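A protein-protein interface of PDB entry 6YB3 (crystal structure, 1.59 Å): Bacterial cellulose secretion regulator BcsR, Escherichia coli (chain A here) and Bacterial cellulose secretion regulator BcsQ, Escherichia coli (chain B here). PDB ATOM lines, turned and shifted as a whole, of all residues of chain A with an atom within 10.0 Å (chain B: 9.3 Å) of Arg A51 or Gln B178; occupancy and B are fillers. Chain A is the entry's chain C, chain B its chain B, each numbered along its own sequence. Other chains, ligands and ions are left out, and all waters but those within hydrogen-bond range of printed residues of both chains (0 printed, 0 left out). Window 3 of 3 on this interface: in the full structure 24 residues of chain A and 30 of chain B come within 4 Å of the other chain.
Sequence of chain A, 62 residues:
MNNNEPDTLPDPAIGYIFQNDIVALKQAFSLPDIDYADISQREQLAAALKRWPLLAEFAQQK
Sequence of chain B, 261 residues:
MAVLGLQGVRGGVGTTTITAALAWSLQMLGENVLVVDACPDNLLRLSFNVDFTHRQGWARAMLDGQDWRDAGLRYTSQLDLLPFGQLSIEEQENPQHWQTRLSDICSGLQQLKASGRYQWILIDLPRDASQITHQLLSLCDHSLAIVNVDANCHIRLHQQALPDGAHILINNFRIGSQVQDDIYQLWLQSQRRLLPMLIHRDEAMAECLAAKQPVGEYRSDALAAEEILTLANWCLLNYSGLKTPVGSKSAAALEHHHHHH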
ATOM      1  N   ARG A  42     -10.842 -23.188  13.057  1.00  0.00           N
ATOM      2  CA  ARG A  42     -11.552 -22.078  13.674  1.00  0.00           C
ATOM      3  C   ARG A  42     -13.045 -22.254  13.428  1.00  0.00           C
ATOM      4  O   ARG A  42     -13.481 -22.382  12.279  1.00  0.00           O
ATOM      5  CB  ARG A  42     -11.053 -20.741  13.125  1.00  0.00           C
ATOM      6  CG  ARG A  42      -9.566 -20.507  13.358  1.00  0.00           C
ATOM      7  CD  ARG A  42      -9.121 -19.157  12.819  1.00  0.00           C
ATOM      8  NE  ARG A  42      -9.635 -18.049  13.620  1.00  0.00           N
ATOM      9  CZ  ARG A  42      -8.946 -17.441  14.581  1.00  0.00           C
ATOM     10  NH1 ARG A  42      -7.709 -17.829  14.860  1.00  0.00           N
ATOM     11  NH2 ARG A  42      -9.493 -16.441  15.260  1.00  0.00           N
ATOM     12  N   GLU A  43     -13.824 -22.270  14.514  1.00  0.00           N
ATOM     13  CA  GLU A  43     -15.263 -22.468  14.388  1.00  0.00           C
ATOM     14  C   GLU A  43     -15.943 -21.241  13.805  1.00  0.00           C
ATOM     15  O   GLU A  43     -16.995 -21.363  13.167  1.00  0.00           O
ATOM     16  CB  GLU A  43     -15.869 -22.811  15.749  1.00  0.00           C
ATOM     17  CG  GLU A  43     -17.150 -23.626  15.673  1.00  0.00           C
ATOM     18  CD  GLU A  43     -16.902 -25.061  15.239  1.00  0.00           C
ATOM     19  OE1 GLU A  43     -16.608 -25.289  14.046  1.00  0.00           O
ATOM     20  OE2 GLU A  43     -16.991 -25.963  16.100  1.00  0.00           O
ATOM     21  N   GLN A  44     -15.367 -20.059  14.023  1.00  0.00           N
ATOM     22  CA  GLN A  44     -15.899 -18.847  13.415  1.00  0.00           C
ATOM     23  C   GLN A  44     -15.911 -18.943  11.897  1.00  0.00           C
ATOM     24  O   GLN A  44     -16.827 -18.422  11.249  1.00  0.00           O
ATOM     25  CB  GLN A  44     -15.075 -17.645  13.868  1.00  0.00           C
ATOM     26  CG  GLN A  44     -14.846 -17.607  15.372  1.00  0.00           C
ATOM     27  CD  GLN A  44     -13.445 -17.162  15.739  1.00  0.00           C
ATOM     28  OE1 GLN A  44     -12.622 -16.873  14.869  1.00  0.00           O
ATOM     29  NE2 GLN A  44     -13.167 -17.106  17.037  1.00  0.00           N
ATOM     30  N   LEU A  45     -14.915 -19.615  11.312  1.00  0.00           N
ATOM     31  CA  LEU A  45     -14.890 -19.786   9.866  1.00  0.00           C
ATOM     32  C   LEU A  45     -15.808 -20.909   9.411  1.00  0.00           C
ATOM     33  O   LEU A  45     -16.341 -20.849   8.299  1.00  0.00           O
ATOM     34  CB  LEU A  45     -13.464 -20.052   9.387  1.00  0.00           C
ATOM     35  CG  LEU A  45     -12.487 -18.891   9.553  1.00  0.00           C
ATOM     36  CD1 LEU A  45     -11.187 -19.163   8.802  1.00  0.00           C
ATOM     37  CD2 LEU A  45     -13.124 -17.595   9.077  1.00  0.00           C
ATOM     38  N   ALA A  46     -16.004 -21.935  10.240  1.00  0.00           N
ATOM     39  CA  ALA A  46     -16.895 -23.022   9.849  1.00  0.00           C
ATOM     40  C   ALA A  46     -18.327 -22.524   9.681  1.00  0.00           C
ATOM     41  O   ALA A  46     -19.039 -22.954   8.765  1.00  0.00           O
ATOM     42  CB  ALA A  46     -16.827 -24.152  10.874  1.00  0.00           C
ATOM     43  N   ALA A  47     -18.760 -21.606  10.551  1.00  0.00           N
ATOM     44  CA  ALA A  47     -20.100 -21.042  10.434  1.00  0.00           C
ATOM     45  C   ALA A  47     -20.219 -20.157   9.198  1.00  0.00           C
ATOM     46  O   ALA A  47     -21.205 -20.239   8.454  1.00  0.00           O
ATOM     47  CB  ALA A  47     -20.447 -20.255  11.698  1.00  0.00           C
ATOM     48  N   ALA A  48     -19.222 -19.297   8.964  1.00  0.00           N
ATOM     49  CA  ALA A  48     -19.234 -18.463   7.767  1.00  0.00           C
ATOM     50  C   ALA A  48     -19.258 -19.313   6.503  1.00  0.00           C
ATOM     51  O   ALA A  48     -19.935 -18.966   5.526  1.00  0.00           O
ATOM     52  CB  ALA A  48     -18.024 -17.531   7.760  1.00  0.00           C
ATOM     53  N   LEU A  49     -18.523 -20.429   6.496  1.00  0.00           N
ATOM     54  CA  LEU A  49     -18.547 -21.304   5.328  1.00  0.00           C
ATOM     55  C   LEU A  49     -19.919 -21.933   5.138  1.00  0.00           C
ATOM     56  O   LEU A  49     -20.339 -22.169   4.000  1.00  0.00           O
ATOM     57  CB  LEU A  49     -17.479 -22.394   5.441  1.00  0.00           C
ATOM     58  CG  LEU A  49     -16.004 -22.014   5.264  1.00  0.00           C
ATOM     59  CD1 LEU A  49     -15.155 -23.266   5.139  1.00  0.00           C
ATOM     60  CD2 LEU A  49     -15.793 -21.105   4.069  1.00  0.00           C
ATOM     61  N   LYS A  50     -20.635 -22.193   6.233  1.00  0.00           N
ATOM     62  CA  LYS A  50     -21.981 -22.739   6.134  1.00  0.00           C
ATOM     63  C   LYS A  50     -22.993 -21.693   5.676  1.00  0.00           C
ATOM     64  O   LYS A  50     -23.958 -22.034   4.988  1.00  0.00           O
ATOM     65  CB  LYS A  50     -22.400 -23.335   7.481  1.00  0.00           C
ATOM     66  CG  LYS A  50     -23.669 -24.175   7.423  1.00  0.00           C
ATOM     67  CD  LYS A  50     -23.929 -24.908   8.734  1.00  0.00           C
ATOM     68  CE  LYS A  50     -22.865 -25.962   9.013  1.00  0.00           C
ATOM     69  NZ  LYS A  50     -23.241 -26.851  10.150  1.00  0.00           N
ATOM     70  N   ARG A  51     -22.791 -20.426   6.054  1.00  0.00           N
ATOM     71  CA  ARG A  51     -23.710 -19.365   5.645  1.00  0.00           C
ATOM     72  C   ARG A  51     -23.638 -19.107   4.144  1.00  0.00           C
ATOM     73  O   ARG A  51     -24.663 -18.853   3.501  1.00  0.00           O
ATOM     74  CB  ARG A  51     -23.403 -18.068   6.403  1.00  0.00           C
ATOM     75  CG  ARG A  51     -23.690 -18.088   7.902  1.00  0.00           C
ATOM     76  CD  ARG A  51     -23.684 -16.668   8.482  1.00  0.00           C
ATOM     77  NE  ARG A  51     -22.350 -16.196   8.854  1.00  0.00           N
ATOM     78  CZ  ARG A  51     -21.795 -16.439  10.037  1.00  0.00           C
ATOM     79  NH1 ARG A  51     -20.582 -15.981  10.322  1.00  0.00           N
ATOM     80  NH2 ARG A  51     -22.461 -17.147  10.938  1.00  0.00           N
ATOM     81  N   TRP A  52     -22.439 -19.157   3.572  1.00  0.00           N
ATOM     82  CA  TRP A  52     -22.202 -18.697   2.201  1.00  0.00           C
ATOM     83  C   TRP A  52     -21.660 -19.805   1.313  1.00  0.00           C
ATOM     84  O   TRP A  52     -20.448 -20.093   1.344  1.00  0.00           O
ATOM     85  CB  TRP A  52     -21.235 -17.510   2.208  1.00  0.00           C
ATOM     86  CG  TRP A  52     -21.637 -16.436   3.163  1.00  0.00           C
ATOM     87  CD1 TRP A  52     -20.926 -15.987   4.248  1.00  0.00           C
ATOM     88  CD2 TRP A  52     -22.853 -15.680   3.144  1.00  0.00           C
ATOM     89  NE1 TRP A  52     -21.619 -14.995   4.889  1.00  0.00           N
ATOM     90  CE2 TRP A  52     -22.804 -14.784   4.235  1.00  0.00           C
ATOM     91  CE3 TRP A  52     -23.975 -15.665   2.304  1.00  0.00           C
ATOM     92  CZ2 TRP A  52     -23.844 -13.894   4.518  1.00  0.00           C
ATOM     93  CZ3 TRP A  52     -25.004 -14.781   2.587  1.00  0.00           C
ATOM     94  CH2 TRP A  52     -24.933 -13.913   3.689  1.00  0.00           C
ATOM     95  N   PRO A  53     -22.497 -20.419   0.468  1.00  0.00           N
ATOM     96  CA  PRO A  53     -21.994 -21.481  -0.425  1.00  0.00           C
ATOM     97  C   PRO A  53     -20.835 -21.057  -1.321  1.00  0.00           C
ATOM     98  O   PRO A  53     -19.987 -21.899  -1.650  1.00  0.00           O
ATOM     99  CB  PRO A  53     -23.234 -21.859  -1.255  1.00  0.00           C
ATOM    100  CG  PRO A  53     -24.172 -20.691  -1.114  1.00  0.00           C
ATOM    101  CD  PRO A  53     -23.932 -20.149   0.264  1.00  0.00           C
ATOM    102  N   LEU A  54     -20.760 -19.786  -1.733  1.00  0.00           N
ATOM    103  CA  LEU A  54     -19.640 -19.351  -2.574  1.00  0.00           C
ATOM    104  C   LEU A  54     -18.308 -19.509  -1.852  1.00  0.00           C
ATOM    105  O   LEU A  54     -17.318 -19.956  -2.447  1.00  0.00           O
ATOM    106  CB  LEU A  54     -19.826 -17.897  -3.006  1.00  0.00           C
ATOM    107  CG  LEU A  54     -18.766 -17.315  -3.951  1.00  0.00           C
ATOM    108  CD1 LEU A  54     -18.910 -17.861  -5.388  1.00  0.00           C
ATOM    109  CD2 LEU A  54     -18.823 -15.790  -3.930  1.00  0.00           C
ATOM    110  N   LEU A  55     -18.256 -19.139  -0.569  1.00  0.00           N
ATOM    111  CA  LEU A  55     -17.022 -19.316   0.188  1.00  0.00           C
ATOM    112  C   LEU A  55     -16.702 -20.792   0.383  1.00  0.00           C
ATOM    113  O   LEU A  55     -15.535 -21.195   0.305  1.00  0.00           O
ATOM    114  CB  LEU A  55     -17.124 -18.604   1.536  1.00  0.00           C
ATOM    115  CG  LEU A  55     -17.486 -17.117   1.473  1.00  0.00           C
ATOM    116  CD1 LEU A  55     -17.371 -16.474   2.853  1.00  0.00           C
ATOM    117  CD2 LEU A  55     -16.629 -16.378   0.475  1.00  0.00           C
ATOM    118  N   ALA A  56     -17.723 -21.613   0.643  1.00  0.00           N
ATOM    119  CA  ALA A  56     -17.495 -23.048   0.782  1.00  0.00           C
ATOM    120  C   ALA A  56     -16.929 -23.640  -0.503  1.00  0.00           C
ATOM    121  O   ALA A  56     -16.038 -24.496  -0.462  1.00  0.00           O
ATOM    122  CB  ALA A  56     -18.795 -23.757   1.168  1.00  0.00           C
ATOM    123  N   GLU A  57     -17.426 -23.176  -1.650  1.00  0.00           N
ATOM    124  CA  GLU A  57     -17.013 -23.717  -2.941  1.00  0.00           C
ATOM    125  C   GLU A  57     -15.503 -23.609  -3.146  1.00  0.00           C
ATOM    126  O   GLU A  57     -14.848 -24.578  -3.547  1.00  0.00           O
ATOM    127  CB  GLU A  57     -17.765 -22.980  -4.047  1.00  0.00           C
ATOM    128  CG  GLU A  57     -17.622 -23.564  -5.424  1.00  0.00           C
ATOM    129  CD  GLU A  57     -18.458 -22.806  -6.431  1.00  0.00           C
ATOM    130  OE1 GLU A  57     -18.867 -21.663  -6.122  1.00  0.00           O
ATOM    131  OE2 GLU A  57     -18.712 -23.353  -7.522  1.00  0.00           O
ATOM    132  N   VAL B 149     -13.392  -5.750   0.319  1.00  0.00           N
ATOM    133  CA  VAL B 149     -13.759  -7.065   0.832  1.00  0.00           C
ATOM    134  C   VAL B 149     -15.205  -7.358   0.452  1.00  0.00           C
ATOM    135  O   VAL B 149     -16.144  -7.005   1.177  1.00  0.00           O
ATOM    136  CB  VAL B 149     -13.527  -7.169   2.347  1.00  0.00           C
ATOM    137  CG1 VAL B 149     -13.843  -8.577   2.815  1.00  0.00           C
ATOM    138  CG2 VAL B 149     -12.065  -6.807   2.660  1.00  0.00           C
ATOM    139  N   PHE B 173     -13.204  -0.664   3.824  1.00  0.00           N
ATOM    140  CA  PHE B 173     -13.748  -1.556   4.839  1.00  0.00           C
ATOM    141  C   PHE B 173     -14.828  -0.813   5.622  1.00  0.00           C
ATOM    142  O   PHE B 173     -14.622   0.340   6.012  1.00  0.00           O
ATOM    143  CB  PHE B 173     -12.613  -2.020   5.764  1.00  0.00           C
ATOM    144  CG  PHE B 173     -12.927  -3.287   6.520  1.00  0.00           C
ATOM    145  CD1 PHE B 173     -12.813  -4.523   5.898  1.00  0.00           C
ATOM    146  CD2 PHE B 173     -13.313  -3.243   7.846  1.00  0.00           C
ATOM    147  CE1 PHE B 173     -13.088  -5.687   6.582  1.00  0.00           C
ATOM    148  CE2 PHE B 173     -13.585  -4.407   8.532  1.00  0.00           C
ATOM    149  CZ  PHE B 173     -13.462  -5.630   7.903  1.00  0.00           C
ATOM    150  N   ARG B 174     -15.997  -1.431   5.828  1.00  0.00           N
ATOM    151  CA  ARG B 174     -17.066  -0.684   6.477  1.00  0.00           C
ATOM    152  C   ARG B 174     -17.690  -1.442   7.642  1.00  0.00           C
ATOM    153  O   ARG B 174     -17.471  -2.641   7.844  1.00  0.00           O
ATOM    154  CB  ARG B 174     -18.160  -0.286   5.483  1.00  0.00           C
ATOM    155  CG  ARG B 174     -18.775  -1.421   4.724  1.00  0.00           C
ATOM    156  CD  ARG B 174     -19.748  -0.839   3.695  1.00  0.00           C
ATOM    157  NE  ARG B 174     -20.325  -1.848   2.816  1.00  0.00           N
ATOM    158  CZ  ARG B 174     -21.371  -2.602   3.132  1.00  0.00           C
ATOM    159  NH1 ARG B 174     -21.949  -2.467   4.320  1.00  0.00           N
ATOM    160  NH2 ARG B 174     -21.839  -3.494   2.261  1.00  0.00           N
ATOM    161  N   ILE B 175     -18.459  -0.689   8.422  1.00  0.00           N
ATOM    162  CA  ILE B 175     -19.327  -1.252   9.446  1.00  0.00           C
ATOM    163  C   ILE B 175     -20.630  -1.676   8.783  1.00  0.00           C
ATOM    164  O   ILE B 175     -21.049  -1.096   7.774  1.00  0.00           O
ATOM    165  CB  ILE B 175     -19.588  -0.231  10.573  1.00  0.00           C
ATOM    166  CG1 ILE B 175     -18.278   0.321  11.128  1.00  0.00           C
ATOM    167  CG2 ILE B 175     -20.449  -0.858  11.698  1.00  0.00           C
ATOM    168  CD1 ILE B 175     -17.334  -0.743  11.661  1.00  0.00           C
ATOM    169  N   GLY B 176     -21.265  -2.704   9.342  1.00  0.00           N
ATOM    170  CA  GLY B 176     -22.605  -3.094   8.942  1.00  0.00           C
ATOM    171  C   GLY B 176     -22.729  -4.205   7.927  1.00  0.00           C
ATOM    172  O   GLY B 176     -23.803  -4.342   7.323  1.00  0.00           O
ATOM    173  N   SER B 177     -21.704  -5.027   7.736  1.00  0.00           N
ATOM    174  CA  SER B 177     -21.764  -6.053   6.690  1.00  0.00           C
ATOM    175  C   SER B 177     -21.270  -7.398   7.207  1.00  0.00           C
ATOM    176  O   SER B 177     -20.060  -7.627   7.294  1.00  0.00           O
ATOM    177  CB  SER B 177     -20.968  -5.629   5.469  1.00  0.00           C
ATOM    178  OG  SER B 177     -21.055  -6.614   4.443  1.00  0.00           O
ATOM    179  N   GLN B 178     -22.207  -8.298   7.514  1.00  0.00           N
ATOM    180  CA  GLN B 178     -21.812  -9.628   7.959  1.00  0.00           C
ATOM    181  C   GLN B 178     -21.020 -10.362   6.884  1.00  0.00           C
ATOM    182  O   GLN B 178     -20.018 -11.021   7.185  1.00  0.00           O
ATOM    183  CB  GLN B 178     -23.034 -10.451   8.364  1.00  0.00           C
ATOM    184  CG  GLN B 178     -22.661 -11.831   8.913  1.00  0.00           C
ATOM    185  CD  GLN B 178     -21.870 -11.778  10.212  1.00  0.00           C
ATOM    186  OE1 GLN B 178     -22.126 -10.941  11.079  1.00  0.00           O
ATOM    187  NE2 GLN B 178     -20.905 -12.678  10.355  1.00  0.00           N
ATOM    188  N   VAL B 179     -21.461 -10.289   5.629  1.00  0.00           N
ATOM    189  CA  VAL B 179     -20.753 -11.052   4.609  1.00  0.00           C
ATOM    190  C   VAL B 179     -19.333 -10.515   4.422  1.00  0.00           C
ATOM    191  O   VAL B 179     -18.388 -11.293   4.258  1.00  0.00           O
ATOM    192  CB  VAL B 179     -21.569 -11.090   3.301  1.00  0.00           C
ATOM    193  CG1 VAL B 179     -21.697  -9.706   2.654  1.00  0.00           C
ATOM    194  CG2 VAL B 179     -20.965 -12.104   2.318  1.00  0.00           C
ATOM    195  N   GLN B 180     -19.145  -9.193   4.498  1.00  0.00           N
ATOM    196  CA  GLN B 180     -17.784  -8.644   4.488  1.00  0.00           C
ATOM    197  C   GLN B 180     -16.972  -9.192   5.652  1.00  0.00           C
ATOM    198  O   GLN B 180     -15.847  -9.671   5.466  1.00  0.00           O
ATOM    199  CB  GLN B 180     -17.811  -7.118   4.557  1.00  0.00           C
ATOM    200  CG  GLN B 180     -16.424  -6.480   4.704  1.00  0.00           C
ATOM    201  CD  GLN B 180     -16.517  -5.112   5.347  1.00  0.00           C
ATOM    202  OE1 GLN B 180     -16.424  -4.088   4.663  1.00  0.00           O
ATOM    203  NE2 GLN B 180     -16.718  -5.085   6.670  1.00  0.00           N
ATOM    204  N   ASP B 181     -17.545  -9.159   6.862  1.00  0.00           N
ATOM    205  CA  ASP B 181     -16.828  -9.651   8.035  1.00  0.00           C
ATOM    206  C   ASP B 181     -16.445 -11.115   7.871  1.00  0.00           C
ATOM    207  O   ASP B 181     -15.353 -11.529   8.287  1.00  0.00           O
ATOM    208  CB  ASP B 181     -17.682  -9.449   9.292  1.00  0.00           C
ATOM    209  CG  ASP B 181     -17.866  -7.979   9.638  1.00  0.00           C
ATOM    210  OD1 ASP B 181     -17.160  -7.135   9.056  1.00  0.00           O
ATOM    211  OD2 ASP B 181     -18.713  -7.662  10.499  1.00  0.00           O
ATOM    212  N   ASP B 182     -17.324 -11.912   7.253  1.00  0.00           N
ATOM    213  CA  ASP B 182     -17.034 -13.327   7.054  1.00  0.00           C
ATOM    214  C   ASP B 182     -15.914 -13.518   6.043  1.00  0.00           C
ATOM    215  O   ASP B 182     -15.008 -14.332   6.254  1.00  0.00           O
ATOM    216  CB  ASP B 182     -18.287 -14.062   6.581  1.00  0.00           C
ATOM    217  CG  ASP B 182     -19.305 -14.261   7.684  1.00  0.00           C
ATOM    218  OD1 ASP B 182     -18.908 -14.248   8.866  1.00  0.00           O
ATOM    219  OD2 ASP B 182     -20.504 -14.442   7.352  1.00  0.00           O
ATOM    220  N   ILE B 183     -15.983 -12.795   4.922  1.00  0.00           N
ATOM    221  CA  ILE B 183     -14.940 -12.886   3.908  1.00  0.00           C
ATOM    222  C   ILE B 183     -13.612 -12.443   4.492  1.00  0.00           C
ATOM    223  O   ILE B 183     -12.586 -13.101   4.306  1.00  0.00           O
ATOM    224  CB  ILE B 183     -15.318 -12.055   2.665  1.00  0.00           C
ATOM    225  CG1 ILE B 183     -16.521 -12.672   1.942  1.00  0.00           C
ATOM    226  CG2 ILE B 183     -14.121 -11.936   1.695  1.00  0.00           C
ATOM    227  CD1 ILE B 183     -17.059 -11.794   0.801  1.00  0.00           C
ATOM    228  N   TYR B 184     -13.631 -11.347   5.256  1.00  0.00           N
ATOM    229  CA  TYR B 184     -12.411 -10.826   5.861  1.00  0.00           C
ATOM    230  C   TYR B 184     -11.785 -11.832   6.819  1.00  0.00           C
ATOM    231  O   TYR B 184     -10.569 -12.050   6.790  1.00  0.00           O
ATOM    232  CB  TYR B 184     -12.724  -9.504   6.564  1.00  0.00           C
ATOM    233  CG  TYR B 184     -11.577  -8.940   7.361  1.00  0.00           C
ATOM    234  CD1 TYR B 184     -10.434  -8.472   6.732  1.00  0.00           C
ATOM    235  CD2 TYR B 184     -11.659  -8.855   8.738  1.00  0.00           C
ATOM    236  CE1 TYR B 184      -9.374  -7.947   7.479  1.00  0.00           C
ATOM    237  CE2 TYR B 184     -10.627  -8.336   9.474  1.00  0.00           C
ATOM    238  CZ  TYR B 184      -9.496  -7.888   8.847  1.00  0.00           C
ATOM    239  OH  TYR B 184      -8.478  -7.371   9.627  1.00  0.00           O
ATOM    240  N   GLN B 185     -12.597 -12.477   7.662  1.00  0.00           N
ATOM    241  CA  GLN B 185     -12.034 -13.459   8.585  1.00  0.00           C
ATOM    242  C   GLN B 185     -11.436 -14.641   7.830  1.00  0.00           C
ATOM    243  O   GLN B 185     -10.396 -15.179   8.229  1.00  0.00           O
ATOM    244  CB  GLN B 185     -13.097 -13.925   9.582  1.00  0.00           C
ATOM    245  CG  GLN B 185     -13.475 -12.859  10.604  1.00  0.00           C
ATOM    246  CD  GLN B 185     -12.284 -12.386  11.437  1.00  0.00           C
ATOM    247  OE1 GLN B 185     -11.394 -13.171  11.776  1.00  0.00           O
ATOM    248  NE2 GLN B 185     -12.265 -11.096  11.764  1.00  0.00           N
ATOM    249  N   LEU B 186     -12.085 -15.065   6.744  1.00  0.00           N
ATOM    250  CA  LEU B 186     -11.524 -16.129   5.920  1.00  0.00           C
ATOM    251  C   LEU B 186     -10.212 -15.697   5.273  1.00  0.00           C
ATOM    252  O   LEU B 186      -9.250 -16.474   5.233  1.00  0.00           O
ATOM    253  CB  LEU B 186     -12.539 -16.542   4.853  1.00  0.00           C
ATOM    254  CG  LEU B 186     -12.133 -17.608   3.831  1.00  0.00           C
ATOM    255  CD1 LEU B 186     -11.750 -18.901   4.525  1.00  0.00           C
ATOM    256  CD2 LEU B 186     -13.290 -17.860   2.877  1.00  0.00           C
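The side-chain carboxylate (OD1) of Asp B182 lies within salt-bridge range of the guanidinium group (NH1) of Arg A51, 2.8 Å away. The side-chain amide nitrogen of Gln B178 lies close to the guanidinium group of Arg A51 (3.3 Å). The side-chain carboxylate (OD2) of Asp B182 is in hydrogen-bond range of the indole nitrogen (NE1) of Trp A52 (2.8 Å).
The side-chain amide nitrogen (NE2) of Gln B178 is in hydrogen-bond range of the side-chain carboxylate (OD1) of Asp B182 (2.9 Å).
Leu A45 touches Gln B185. Leu A45 touches Leu B186. CG of Asp B182 touches CB of Ala A48 (3.5 Å). Trp A52 touches Val B179 (CE2 to CG2, 3.8 Å). Leu A55 touches Ile B183 (CD2 to CG1, 3.99 Å).
Printed residues of chain B within 4 Å of Arg A51: Gln B178 (3.3 Å) and Asp B182 (2.8 Å). Printed residues of chain A within 4 Å of Gln B178: Arg A51. Ala A48 touches just one residue of chain B: Asp B182. Trp A52 touches just these residues of chain B: Val B179 and Asp B182. No residue of chain A comes within 4 Å of Ser B177. Val B179 touches one residue of chain A. Printed residues of chain B within 4 Å of Leu A55: Ile B183 (3.99 Å). Of the printed residues of chain B, Leu A45 touches Gln B185 and Leu B186. Of the printed residues of chain A, Asp B182 touches Ala A48 (3.5 Å), Arg A51 (2.8 Å) and Trp A52 (2.8 Å). Of the printed residues of chain A, Gln B185 touches Leu A45 (3.6 Å). Ala A47 touches none of the printed residues of chain B. Arg B174 touches none of the printed residues of chain A. The nearest printed residue of chain B that does not touch Arg A51 is Val B179 (6.8 Å).
Of the 16 printed residues of chain A, 5 touch a printed residue of chain B. Among the printed residues, 8 pairs touch across the chains. Among the printed residues, Asp or Glu carboxylates within 4 Å of a Lys or Arg side-chain nitrogen of the other chain: Arg A51 with Asp B182.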
